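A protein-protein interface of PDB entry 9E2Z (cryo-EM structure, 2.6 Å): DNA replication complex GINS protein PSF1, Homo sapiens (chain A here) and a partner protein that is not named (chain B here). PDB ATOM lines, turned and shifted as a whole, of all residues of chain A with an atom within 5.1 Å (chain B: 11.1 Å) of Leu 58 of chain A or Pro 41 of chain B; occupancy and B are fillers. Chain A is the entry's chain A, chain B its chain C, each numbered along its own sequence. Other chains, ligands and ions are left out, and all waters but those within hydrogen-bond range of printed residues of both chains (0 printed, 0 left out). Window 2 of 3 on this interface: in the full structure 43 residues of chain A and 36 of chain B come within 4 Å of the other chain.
OG1 of Thr 61 of chain A is in hydrogen-bond range of O of Pro 41 of chain B (2.5 Å). OE1 of Glu 49 of chain A lies within salt-bridge range of NH2 of Arg 42 of chain B, at 2.5 Å. The side-chain carboxylate (OD1) of Asp 46 of chain A is in salt-bridge range of the guanidinium group (NH1) of Arg 42 of chain B, 2.7 Å away.
The backbone NH of Met 40 of chain B is in hydrogen-bond range of the backbone carbonyl oxygen of Val 60 of chain B (3.1 Å). N of Leu 43 of chain B is in hydrogen-bond range of O of Asn 58 of chain B. The guanidinium group (NH2) of Arg 55 of chain A is in salt-bridge range of the side-chain carboxylate (OD2) of Asp 57 of chain A (3.0 Å). The backbone NH (N) of Arg 42 of chain B is in hydrogen-bond range of the backbone carbonyl oxygen (O) of Asn 58 of chain B.
Pro 41 of chain B touches Asp 57 of chain A. CD2 of Leu 58 of chain A touches CG of Pro 41 of chain B, at 3.9 Å. NE of Arg 42 of chain B touches CD2 of Leu 58 of chain A, 3.7 Å away. Pro 60 of chain A touches Met 40 of chain B (CB to CG, 3.9 Å). Leu 43 of chain B touches Thr 61 of chain A (CD2 to CG2, 3.6 Å).
Asp 46 of chain A touches one residue of chain B. Of the printed residues of chain B, Glu 49 of chain A touches Arg 42 (2.5 Å). Ala 50 of chain A touches none of the printed residues of chain B. No residue of chain B comes within 4 Å of Arg 55 of chain A. No residue of chain B comes within 4 Å of Ser 56 of chain A. Leu 58 of chain A touches just these residues of chain B: Pro 41 and Arg 42. No residue of chain B comes within 4 Å of Ile 59 of chain A. Of chain B, only Pro 41 and Leu 43 come within 4 Å of Thr 61 of chain A. No residue of chain B comes within 4 Å of Ile 62 of chain A. Of the printed residues of chain A, Met 40 of chain B touches Pro 60 (3.9 Å). Of the printed residues of chain A, Pro 41 of chain B touches Asp 57, Leu 58 and Thr 61. Printed residues of chain A within 4 Å of Arg 42 of chain B: Asp 46, Glu 49 and Leu 58. Of the printed residues of chain A, Leu 43 of chain B touches Thr 61. Phe 47 of chain B touches none of the printed residues of chain A.
Of the 11 printed residues of chain A, 6 touch a printed residue of chain B.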
ATOM      1  N   ASP A  46      29.282  -1.603   6.016  1.00  0.00           N
ATOM      2  CA  ASP A  46      27.976  -2.253   6.062  1.00  0.00           C
ATOM      3  C   ASP A  46      27.521  -2.679   4.671  1.00  0.00           C
ATOM      4  O   ASP A  46      26.965  -3.766   4.501  1.00  0.00           O
ATOM      5  CB  ASP A  46      26.947  -1.317   6.690  1.00  0.00           C
ATOM      6  CG  ASP A  46      26.781  -1.546   8.173  1.00  0.00           C
ATOM      7  OD1 ASP A  46      27.719  -2.074   8.805  1.00  0.00           O
ATOM      8  OD2 ASP A  46      25.711  -1.193   8.708  1.00  0.00           O
ATOM      9  N   GLU A  49      29.432  -5.745   3.515  1.00  0.00           N
ATOM     10  CA  GLU A  49      28.931  -6.941   4.189  1.00  0.00           C
ATOM     11  C   GLU A  49      27.571  -7.354   3.642  1.00  0.00           C
ATOM     12  O   GLU A  49      27.291  -8.548   3.486  1.00  0.00           O
ATOM     13  CB  GLU A  49      28.848  -6.698   5.695  1.00  0.00           C
ATOM     14  CG  GLU A  49      30.114  -7.056   6.443  1.00  0.00           C
ATOM     15  CD  GLU A  49      29.881  -7.237   7.927  1.00  0.00           C
ATOM     16  OE1 GLU A  49      28.708  -7.264   8.350  1.00  0.00           O
ATOM     17  OE2 GLU A  49      30.875  -7.350   8.676  1.00  0.00           O
ATOM     18  N   ALA A  50      26.705  -6.380   3.361  1.00  0.00           N
ATOM     19  CA  ALA A  50      25.392  -6.699   2.818  1.00  0.00           C
ATOM     20  C   ALA A  50      25.518  -7.401   1.477  1.00  0.00           C
ATOM     21  O   ALA A  50      24.804  -8.374   1.205  1.00  0.00           O
ATOM     22  CB  ALA A  50      24.558  -5.425   2.682  1.00  0.00           C
ATOM     23  N   ARG A  55      22.877 -10.148   4.082  1.00  0.00           N
ATOM     24  CA  ARG A  55      22.162  -9.804   5.305  1.00  0.00           C
ATOM     25  C   ARG A  55      21.239  -8.624   5.027  1.00  0.00           C
ATOM     26  O   ARG A  55      21.707  -7.507   4.780  1.00  0.00           O
ATOM     27  CB  ARG A  55      23.136  -9.458   6.428  1.00  0.00           C
ATOM     28  CG  ARG A  55      24.075 -10.584   6.821  1.00  0.00           C
ATOM     29  CD  ARG A  55      25.128 -10.103   7.816  1.00  0.00           C
ATOM     30  NE  ARG A  55      24.584  -9.144   8.774  1.00  0.00           N
ATOM     31  CZ  ARG A  55      24.724  -9.215  10.091  1.00  0.00           C
ATOM     32  NH1 ARG A  55      25.413 -10.186  10.670  1.00  0.00           N
ATOM     33  NH2 ARG A  55      24.160  -8.281  10.853  1.00  0.00           N
ATOM     34  N   SER A  56      19.929  -8.873   5.068  1.00  0.00           N
ATOM     35  CA  SER A  56      18.970  -7.801   4.823  1.00  0.00           C
ATOM     36  C   SER A  56      18.844  -6.873   6.023  1.00  0.00           C
ATOM     37  O   SER A  56      18.555  -5.683   5.854  1.00  0.00           O
ATOM     38  CB  SER A  56      17.606  -8.391   4.470  1.00  0.00           C
ATOM     39  OG  SER A  56      16.626  -7.374   4.362  1.00  0.00           O
ATOM     40  N   ASP A  57      19.074  -7.384   7.233  1.00  0.00           N
ATOM     41  CA  ASP A  57      18.798  -6.604   8.434  1.00  0.00           C
ATOM     42  C   ASP A  57      19.628  -5.330   8.507  1.00  0.00           C
ATOM     43  O   ASP A  57      19.286  -4.428   9.279  1.00  0.00           O
ATOM     44  CB  ASP A  57      19.046  -7.457   9.680  1.00  0.00           C
ATOM     45  CG  ASP A  57      20.374  -8.183   9.635  1.00  0.00           C
ATOM     46  OD1 ASP A  57      20.623  -8.905   8.650  1.00  0.00           O
ATOM     47  OD2 ASP A  57      21.165  -8.038  10.590  1.00  0.00           O
ATOM     48  N   LEU A  58      20.707  -5.229   7.734  1.00  0.00           N
ATOM     49  CA  LEU A  58      21.562  -4.050   7.778  1.00  0.00           C
ATOM     50  C   LEU A  58      21.021  -2.882   6.962  1.00  0.00           C
ATOM     51  O   LEU A  58      21.505  -1.758   7.134  1.00  0.00           O
ATOM     52  CB  LEU A  58      22.966  -4.409   7.283  1.00  0.00           C
ATOM     53  CG  LEU A  58      23.827  -5.278   8.201  1.00  0.00           C
ATOM     54  CD1 LEU A  58      25.186  -5.522   7.578  1.00  0.00           C
ATOM     55  CD2 LEU A  58      23.992  -4.634   9.560  1.00  0.00           C
ATOM     56  N   ILE A  59      20.036  -3.107   6.089  1.00  0.00           N
ATOM     57  CA  ILE A  59      19.569  -2.032   5.207  1.00  0.00           C
ATOM     58  C   ILE A  59      19.025  -0.852   5.997  1.00  0.00           C
ATOM     59  O   ILE A  59      19.351   0.298   5.656  1.00  0.00           O
ATOM     60  CB  ILE A  59      18.563  -2.584   4.188  1.00  0.00           C
ATOM     61  CG1 ILE A  59      19.190  -3.705   3.356  1.00  0.00           C
ATOM     62  CG2 ILE A  59      18.069  -1.477   3.283  1.00  0.00           C
ATOM     63  CD1 ILE A  59      20.364  -3.274   2.504  1.00  0.00           C
ATOM     64  N   PRO A  60      18.190  -1.032   7.023  1.00  0.00           N
ATOM     65  CA  PRO A  60      17.744   0.135   7.798  1.00  0.00           C
ATOM     66  C   PRO A  60      18.890   0.959   8.354  1.00  0.00           C
ATOM     67  O   PRO A  60      18.814   2.193   8.369  1.00  0.00           O
ATOM     68  CB  PRO A  60      16.903  -0.498   8.912  1.00  0.00           C
ATOM     69  CG  PRO A  60      16.395  -1.751   8.320  1.00  0.00           C
ATOM     70  CD  PRO A  60      17.478  -2.258   7.421  1.00  0.00           C
ATOM     71  N   THR A  61      19.960   0.307   8.808  1.00  0.00           N
ATOM     72  CA  THR A  61      21.105   1.043   9.333  1.00  0.00           C
ATOM     73  C   THR A  61      21.778   1.860   8.237  1.00  0.00           C
ATOM     74  O   THR A  61      22.185   3.009   8.466  1.00  0.00           O
ATOM     75  CB  THR A  61      22.094   0.067   9.966  1.00  0.00           C
ATOM     76  OG1 THR A  61      21.402  -0.775  10.897  1.00  0.00           O
ATOM     77  CG2 THR A  61      23.194   0.811  10.694  1.00  0.00           C
ATOM     78  N   ILE A  62      21.900   1.285   7.042  1.00  0.00           N
ATOM     79  CA  ILE A  62      22.482   2.017   5.924  1.00  0.00           C
ATOM     80  C   ILE A  62      21.639   3.242   5.605  1.00  0.00           C
ATOM     81  O   ILE A  62      22.169   4.339   5.383  1.00  0.00           O
ATOM     82  CB  ILE A  62      22.628   1.094   4.699  1.00  0.00           C
ATOM     83  CG1 ILE A  62      23.830   0.169   4.870  1.00  0.00           C
ATOM     84  CG2 ILE A  62      22.797   1.902   3.431  1.00  0.00           C
ATOM     85  CD1 ILE A  62      23.536  -1.261   4.516  1.00  0.00           C
ATOM     86  N   THR B  36       9.165   1.429  16.105  1.00  0.00           N
ATOM     87  CA  THR B  36      10.048   0.764  15.154  1.00  0.00           C
ATOM     88  C   THR B  36       9.411  -0.533  14.673  1.00  0.00           C
ATOM     89  O   THR B  36       9.044  -1.389  15.482  1.00  0.00           O
ATOM     90  CB  THR B  36      11.402   0.490  15.801  1.00  0.00           C
ATOM     91  OG1 THR B  36      11.911   1.699  16.374  1.00  0.00           O
ATOM     92  CG2 THR B  36      12.391  -0.026  14.773  1.00  0.00           C
ATOM     93  N   GLU B  37       9.293  -0.681  13.354  1.00  0.00           N
ATOM     94  CA  GLU B  37       8.635  -1.828  12.747  1.00  0.00           C
ATOM     95  C   GLU B  37       9.611  -2.864  12.202  1.00  0.00           C
ATOM     96  O   GLU B  37       9.186  -3.773  11.483  1.00  0.00           O
ATOM     97  CB  GLU B  37       7.705  -1.363  11.625  1.00  0.00           C
ATOM     98  CG  GLU B  37       6.714  -0.295  12.048  1.00  0.00           C
ATOM     99  CD  GLU B  37       5.861  -0.717  13.223  1.00  0.00           C
ATOM    100  OE1 GLU B  37       5.611  -1.931  13.373  1.00  0.00           O
ATOM    101  OE2 GLU B  37       5.439   0.165  13.997  1.00  0.00           O
ATOM    102  N   THR B  38      10.898  -2.748  12.509  1.00  0.00           N
ATOM    103  CA  THR B  38      11.875  -3.739  12.085  1.00  0.00           C
ATOM    104  C   THR B  38      13.089  -3.649  12.994  1.00  0.00           C
ATOM    105  O   THR B  38      13.453  -2.562  13.447  1.00  0.00           O
ATOM    106  CB  THR B  38      12.296  -3.531  10.627  1.00  0.00           C
ATOM    107  OG1 THR B  38      11.157  -3.677   9.770  1.00  0.00           O
ATOM    108  CG2 THR B  38      13.354  -4.547  10.227  1.00  0.00           C
ATOM    109  N   ALA B  39      13.708  -4.795  13.262  1.00  0.00           N
ATOM    110  CA  ALA B  39      14.946  -4.799  14.025  1.00  0.00           C
ATOM    111  C   ALA B  39      15.991  -3.967  13.296  1.00  0.00           C
ATOM    112  O   ALA B  39      16.085  -4.001  12.067  1.00  0.00           O
ATOM    113  CB  ALA B  39      15.443  -6.229  14.226  1.00  0.00           C
ATOM    114  N   MET B  40      16.780  -3.210  14.058  1.00  0.00           N
ATOM    115  CA  MET B  40      17.697  -2.218  13.500  1.00  0.00           C
ATOM    116  C   MET B  40      19.091  -2.489  14.054  1.00  0.00           C
ATOM    117  O   MET B  40      19.493  -1.896  15.067  1.00  0.00           O
ATOM    118  CB  MET B  40      17.227  -0.805  13.841  1.00  0.00           C
ATOM    119  CG  MET B  40      16.407  -0.148  12.731  1.00  0.00           C
ATOM    120  SD  MET B  40      16.540   1.646  12.630  1.00  0.00           S
ATOM    121  CE  MET B  40      18.294   1.844  12.344  1.00  0.00           C
ATOM    122  N   PRO B  41      19.864  -3.369  13.422  1.00  0.00           N
ATOM    123  CA  PRO B  41      21.163  -3.753  13.983  1.00  0.00           C
ATOM    124  C   PRO B  41      22.191  -2.632  13.936  1.00  0.00           C
ATOM    125  O   PRO B  41      22.121  -1.706  13.127  1.00  0.00           O
ATOM    126  CB  PRO B  41      21.593  -4.930  13.101  1.00  0.00           C
ATOM    127  CG  PRO B  41      20.855  -4.744  11.826  1.00  0.00           C
ATOM    128  CD  PRO B  41      19.556  -4.105  12.184  1.00  0.00           C
ATOM    129  N   ARG B  42      23.163  -2.739  14.843  1.00  0.00           N
ATOM    130  CA  ARG B  42      24.368  -1.910  14.873  1.00  0.00           C
ATOM    131  C   ARG B  42      24.089  -0.452  15.220  1.00  0.00           C
ATOM    132  O   ARG B  42      24.983   0.390  15.099  1.00  0.00           O
ATOM    133  CB  ARG B  42      25.130  -1.992  13.548  1.00  0.00           C
ATOM    134  CG  ARG B  42      25.600  -3.395  13.216  1.00  0.00           C
ATOM    135  CD  ARG B  42      26.593  -3.420  12.074  1.00  0.00           C
ATOM    136  NE  ARG B  42      26.951  -4.788  11.722  1.00  0.00           N
ATOM    137  CZ  ARG B  42      27.902  -5.122  10.861  1.00  0.00           C
ATOM    138  NH1 ARG B  42      28.618  -4.205  10.230  1.00  0.00           N
ATOM    139  NH2 ARG B  42      28.139  -6.409  10.624  1.00  0.00           N
ATOM    140  N   LEU B  43      22.875  -0.129  15.665  1.00  0.00           N
ATOM    141  CA  LEU B  43      22.566   1.207  16.159  1.00  0.00           C
ATOM    142  C   LEU B  43      22.068   1.189  17.598  1.00  0.00           C
ATOM    143  O   LEU B  43      21.587   2.217  18.087  1.00  0.00           O
ATOM    144  CB  LEU B  43      21.520   1.889  15.270  1.00  0.00           C
ATOM    145  CG  LEU B  43      21.909   2.262  13.838  1.00  0.00           C
ATOM    146  CD1 LEU B  43      20.946   3.302  13.321  1.00  0.00           C
ATOM    147  CD2 LEU B  43      23.342   2.764  13.731  1.00  0.00           C
ATOM    148  N   GLY B  44      22.168   0.054  18.289  1.00  0.00           N
ATOM    149  CA  GLY B  44      21.691  -0.012  19.657  1.00  0.00           C
ATOM    150  C   GLY B  44      22.410   0.931  20.598  1.00  0.00           C
ATOM    151  O   GLY B  44      21.818   1.379  21.584  1.00  0.00           O
ATOM    152  N   ALA B  45      23.677   1.243  20.316  1.00  0.00           N
ATOM    153  CA  ALA B  45      24.417   2.163  21.170  1.00  0.00           C
ATOM    154  C   ALA B  45      23.711   3.508  21.288  1.00  0.00           C
ATOM    155  O   ALA B  45      23.732   4.137  22.352  1.00  0.00           O
ATOM    156  CB  ALA B  45      25.837   2.347  20.632  1.00  0.00           C
ATOM    157  N   PHE B  46      23.079   3.972  20.208  1.00  0.00           N
ATOM    158  CA  PHE B  46      22.528   5.321  20.208  1.00  0.00           C
ATOM    159  C   PHE B  46      21.133   5.389  20.817  1.00  0.00           C
ATOM    160  O   PHE B  46      20.593   6.490  20.968  1.00  0.00           O
ATOM    161  CB  PHE B  46      22.487   5.889  18.784  1.00  0.00           C
ATOM    162  CG  PHE B  46      23.784   5.755  18.038  1.00  0.00           C
ATOM    163  CD1 PHE B  46      24.189   4.523  17.555  1.00  0.00           C
ATOM    164  CD2 PHE B  46      24.628   6.836  17.875  1.00  0.00           C
ATOM    165  CE1 PHE B  46      25.382   4.378  16.884  1.00  0.00           C
ATOM    166  CE2 PHE B  46      25.828   6.697  17.204  1.00  0.00           C
ATOM    167  CZ  PHE B  46      26.207   5.463  16.711  1.00  0.00           C
ATOM    168  N   PHE B  47      20.535   4.249  21.156  1.00  0.00           N
ATOM    169  CA  PHE B  47      19.207   4.220  21.762  1.00  0.00           C
ATOM    170  C   PHE B  47      19.126   3.159  22.855  1.00  0.00           C
ATOM    171  O   PHE B  47      19.400   3.437  24.024  1.00  0.00           O
ATOM    172  CB  PHE B  47      18.139   3.960  20.698  1.00  0.00           C
ATOM    173  CG  PHE B  47      18.266   4.838  19.486  1.00  0.00           C
ATOM    174  CD1 PHE B  47      18.057   6.201  19.582  1.00  0.00           C
ATOM    175  CD2 PHE B  47      18.604   4.303  18.255  1.00  0.00           C
ATOM    176  CE1 PHE B  47      18.175   7.015  18.470  1.00  0.00           C
ATOM    177  CE2 PHE B  47      18.725   5.112  17.141  1.00  0.00           C
ATOM    178  CZ  PHE B  47      18.510   6.469  17.250  1.00  0.00           C
ATOM    179  N   ASN B  58      25.026  -4.397  18.757  1.00  0.00           N
ATOM    180  CA  ASN B  58      23.881  -3.874  19.492  1.00  0.00           C
ATOM    181  C   ASN B  58      22.778  -3.465  18.521  1.00  0.00           C
ATOM    182  O   ASN B  58      23.008  -2.672  17.609  1.00  0.00           O
ATOM    183  CB  ASN B  58      24.294  -2.685  20.359  1.00  0.00           C
ATOM    184  CG  ASN B  58      24.957  -3.105  21.665  1.00  0.00           C
ATOM    185  OD1 ASN B  58      24.905  -2.375  22.654  1.00  0.00           O
ATOM    186  ND2 ASN B  58      25.585  -4.277  21.673  1.00  0.00           N
ATOM    187  N   ALA B  59      21.580  -4.010  18.724  1.00  0.00           N
ATOM    188  CA  ALA B  59      20.456  -3.786  17.830  1.00  0.00           C
ATOM    189  C   ALA B  59      19.292  -3.187  18.602  1.00  0.00           C
ATOM    190  O   ALA B  59      19.157  -3.391  19.812  1.00  0.00           O
ATOM    191  CB  ALA B  59      20.007  -5.089  17.151  1.00  0.00           C
ATOM    192  N   VAL B  60      18.458  -2.440  17.890  1.00  0.00           N
ATOM    193  CA  VAL B  60      17.237  -1.861  18.443  1.00  0.00           C
ATOM    194  C   VAL B  60      16.091  -2.821  18.133  1.00  0.00           C
ATOM    195  O   VAL B  60      15.818  -3.074  16.951  1.00  0.00           O
ATOM    196  CB  VAL B  60      16.961  -0.467  17.863  1.00  0.00           C
ATOM    197  CG1 VAL B  60      16.057   0.326  18.794  1.00  0.00           C
ATOM    198  CG2 VAL B  60      18.265   0.278  17.623  1.00  0.00           C
ATOM    199  N   PRO B  61      15.412  -3.374  19.135  1.00  0.00           N
ATOM    200  CA  PRO B  61      14.414  -4.415  18.862  1.00  0.00           C
ATOM    201  C   PRO B  61      13.193  -3.887  18.127  1.00  0.00           C
ATOM    202  O   PRO B  61      12.830  -2.713  18.211  1.00  0.00           O
ATOM    203  CB  PRO B  61      14.037  -4.920  20.258  1.00  0.00           C
ATOM    204  CG  PRO B  61      14.351  -3.791  21.167  1.00  0.00           C
ATOM    205  CD  PRO B  61      15.539  -3.100  20.576  1.00  0.00           C
ATOM    206  N   GLN B  62      12.551  -4.798  17.399  1.00  0.00           N
ATOM    207  CA  GLN B  62      11.288  -4.489  16.744  1.00  0.00           C
ATOM    208  C   GLN B  62      10.250  -4.082  17.784  1.00  0.00           C
ATOM    209  O   GLN B  62      10.213  -4.620  18.893  1.00  0.00           O
ATOM    210  CB  GLN B  62      10.818  -5.710  15.939  1.00  0.00           C
ATOM    211  CG  GLN B  62       9.306  -5.949  15.823  1.00  0.00           C
ATOM    212  CD  GLN B  62       8.719  -5.381  14.549  1.00  0.00           C
ATOM    213  OE1 GLN B  62       9.376  -5.352  13.510  1.00  0.00           O
ATOM    214  NE2 GLN B  62       7.474  -4.925  14.623  1.00  0.00           N
ATOM    215  N   SER B  64      10.080  -1.279  19.353  1.00  0.00           N
ATOM    216  CA  SER B  64      10.568  -0.314  20.324  1.00  0.00           C
ATOM    217  C   SER B  64       9.971   1.063  20.055  1.00  0.00           C
ATOM    218  O   SER B  64       9.592   1.393  18.929  1.00  0.00           O
ATOM    219  CB  SER B  64      12.094  -0.241  20.278  1.00  0.00           C
ATOM    220  OG  SER B  64      12.547   0.240  19.027  1.00  0.00           O
ATOM    221  N   LEU B  66      10.618   5.137  20.288  1.00  0.00           N
ATOM    222  CA  LEU B  66      11.701   6.107  20.307  1.00  0.00           C
ATOM    223  C   LEU B  66      11.166   7.489  19.972  1.00  0.00           C
ATOM    224  O   LEU B  66      10.055   7.643  19.460  1.00  0.00           O
ATOM    225  CB  LEU B  66      12.808   5.743  19.309  1.00  0.00           C
ATOM    226  CG  LEU B  66      13.437   4.358  19.435  1.00  0.00           C
ATOM    227  CD1 LEU B  66      13.277   3.596  18.137  1.00  0.00           C
ATOM    228  CD2 LEU B  66      14.901   4.466  19.811  1.00  0.00           C
ATOM    229  N   LEU B  76      13.289   8.125   7.023  1.00  0.00           N
ATOM    230  CA  LEU B  76      13.049   6.691   7.119  1.00  0.00           C
ATOM    231  C   LEU B  76      11.622   6.291   6.778  1.00  0.00           C
ATOM    232  O   LEU B  76      11.373   5.106   6.544  1.00  0.00           O
ATOM    233  CB  LEU B  76      13.381   6.198   8.528  1.00  0.00           C
ATOM    234  CG  LEU B  76      14.832   6.375   8.971  1.00  0.00           C
ATOM    235  CD1 LEU B  76      14.943   6.225  10.472  1.00  0.00           C
ATOM    236  CD2 LEU B  76      15.729   5.377   8.266  1.00  0.00           C
ATOM    237  N   ARG B  82       7.518   0.331   6.582  1.00  0.00           N
ATOM    238  CA  ARG B  82       8.507  -0.741   6.653  1.00  0.00           C
ATOM    239  C   ARG B  82       9.416  -0.574   7.865  1.00  0.00           C
ATOM    240  O   ARG B  82       9.556  -1.494   8.676  1.00  0.00           O
ATOM    241  CB  ARG B  82       9.362  -0.781   5.380  1.00  0.00           C
ATOM    242  CG  ARG B  82       8.640  -1.176   4.107  1.00  0.00           C
ATOM    243  CD  ARG B  82       9.606  -1.225   2.931  1.00  0.00           C
ATOM    244  NE  ARG B  82       8.929  -1.534   1.676  1.00  0.00           N
ATOM    245  CZ  ARG B  82       9.503  -1.529   0.481  1.00  0.00           C
ATOM    246  NH1 ARG B  82      10.783  -1.236   0.328  1.00  0.00           N
ATOM    247  NH2 ARG B  82       8.773  -1.827  -0.589  1.00  0.00           N
ATOM    248  N   ILE B  83      10.043   0.591   7.993  1.00  0.00           N
ATOM    249  CA  ILE B  83      11.049   0.808   9.026  1.00  0.00           C
ATOM    250  C   ILE B  83      10.424   1.307  10.323  1.00  0.00           C
ATOM    251  O   ILE B  83      10.790   0.850  11.405  1.00  0.00           O
ATOM    252  CB  ILE B  83      12.120   1.785   8.502  1.00  0.00           C
ATOM    253  CG1 ILE B  83      12.722   1.243   7.204  1.00  0.00           C
ATOM    254  CG2 ILE B  83      13.207   2.013   9.549  1.00  0.00           C
ATOM    255  CD1 ILE B  83      14.127   1.721   6.914  1.00  0.00           C
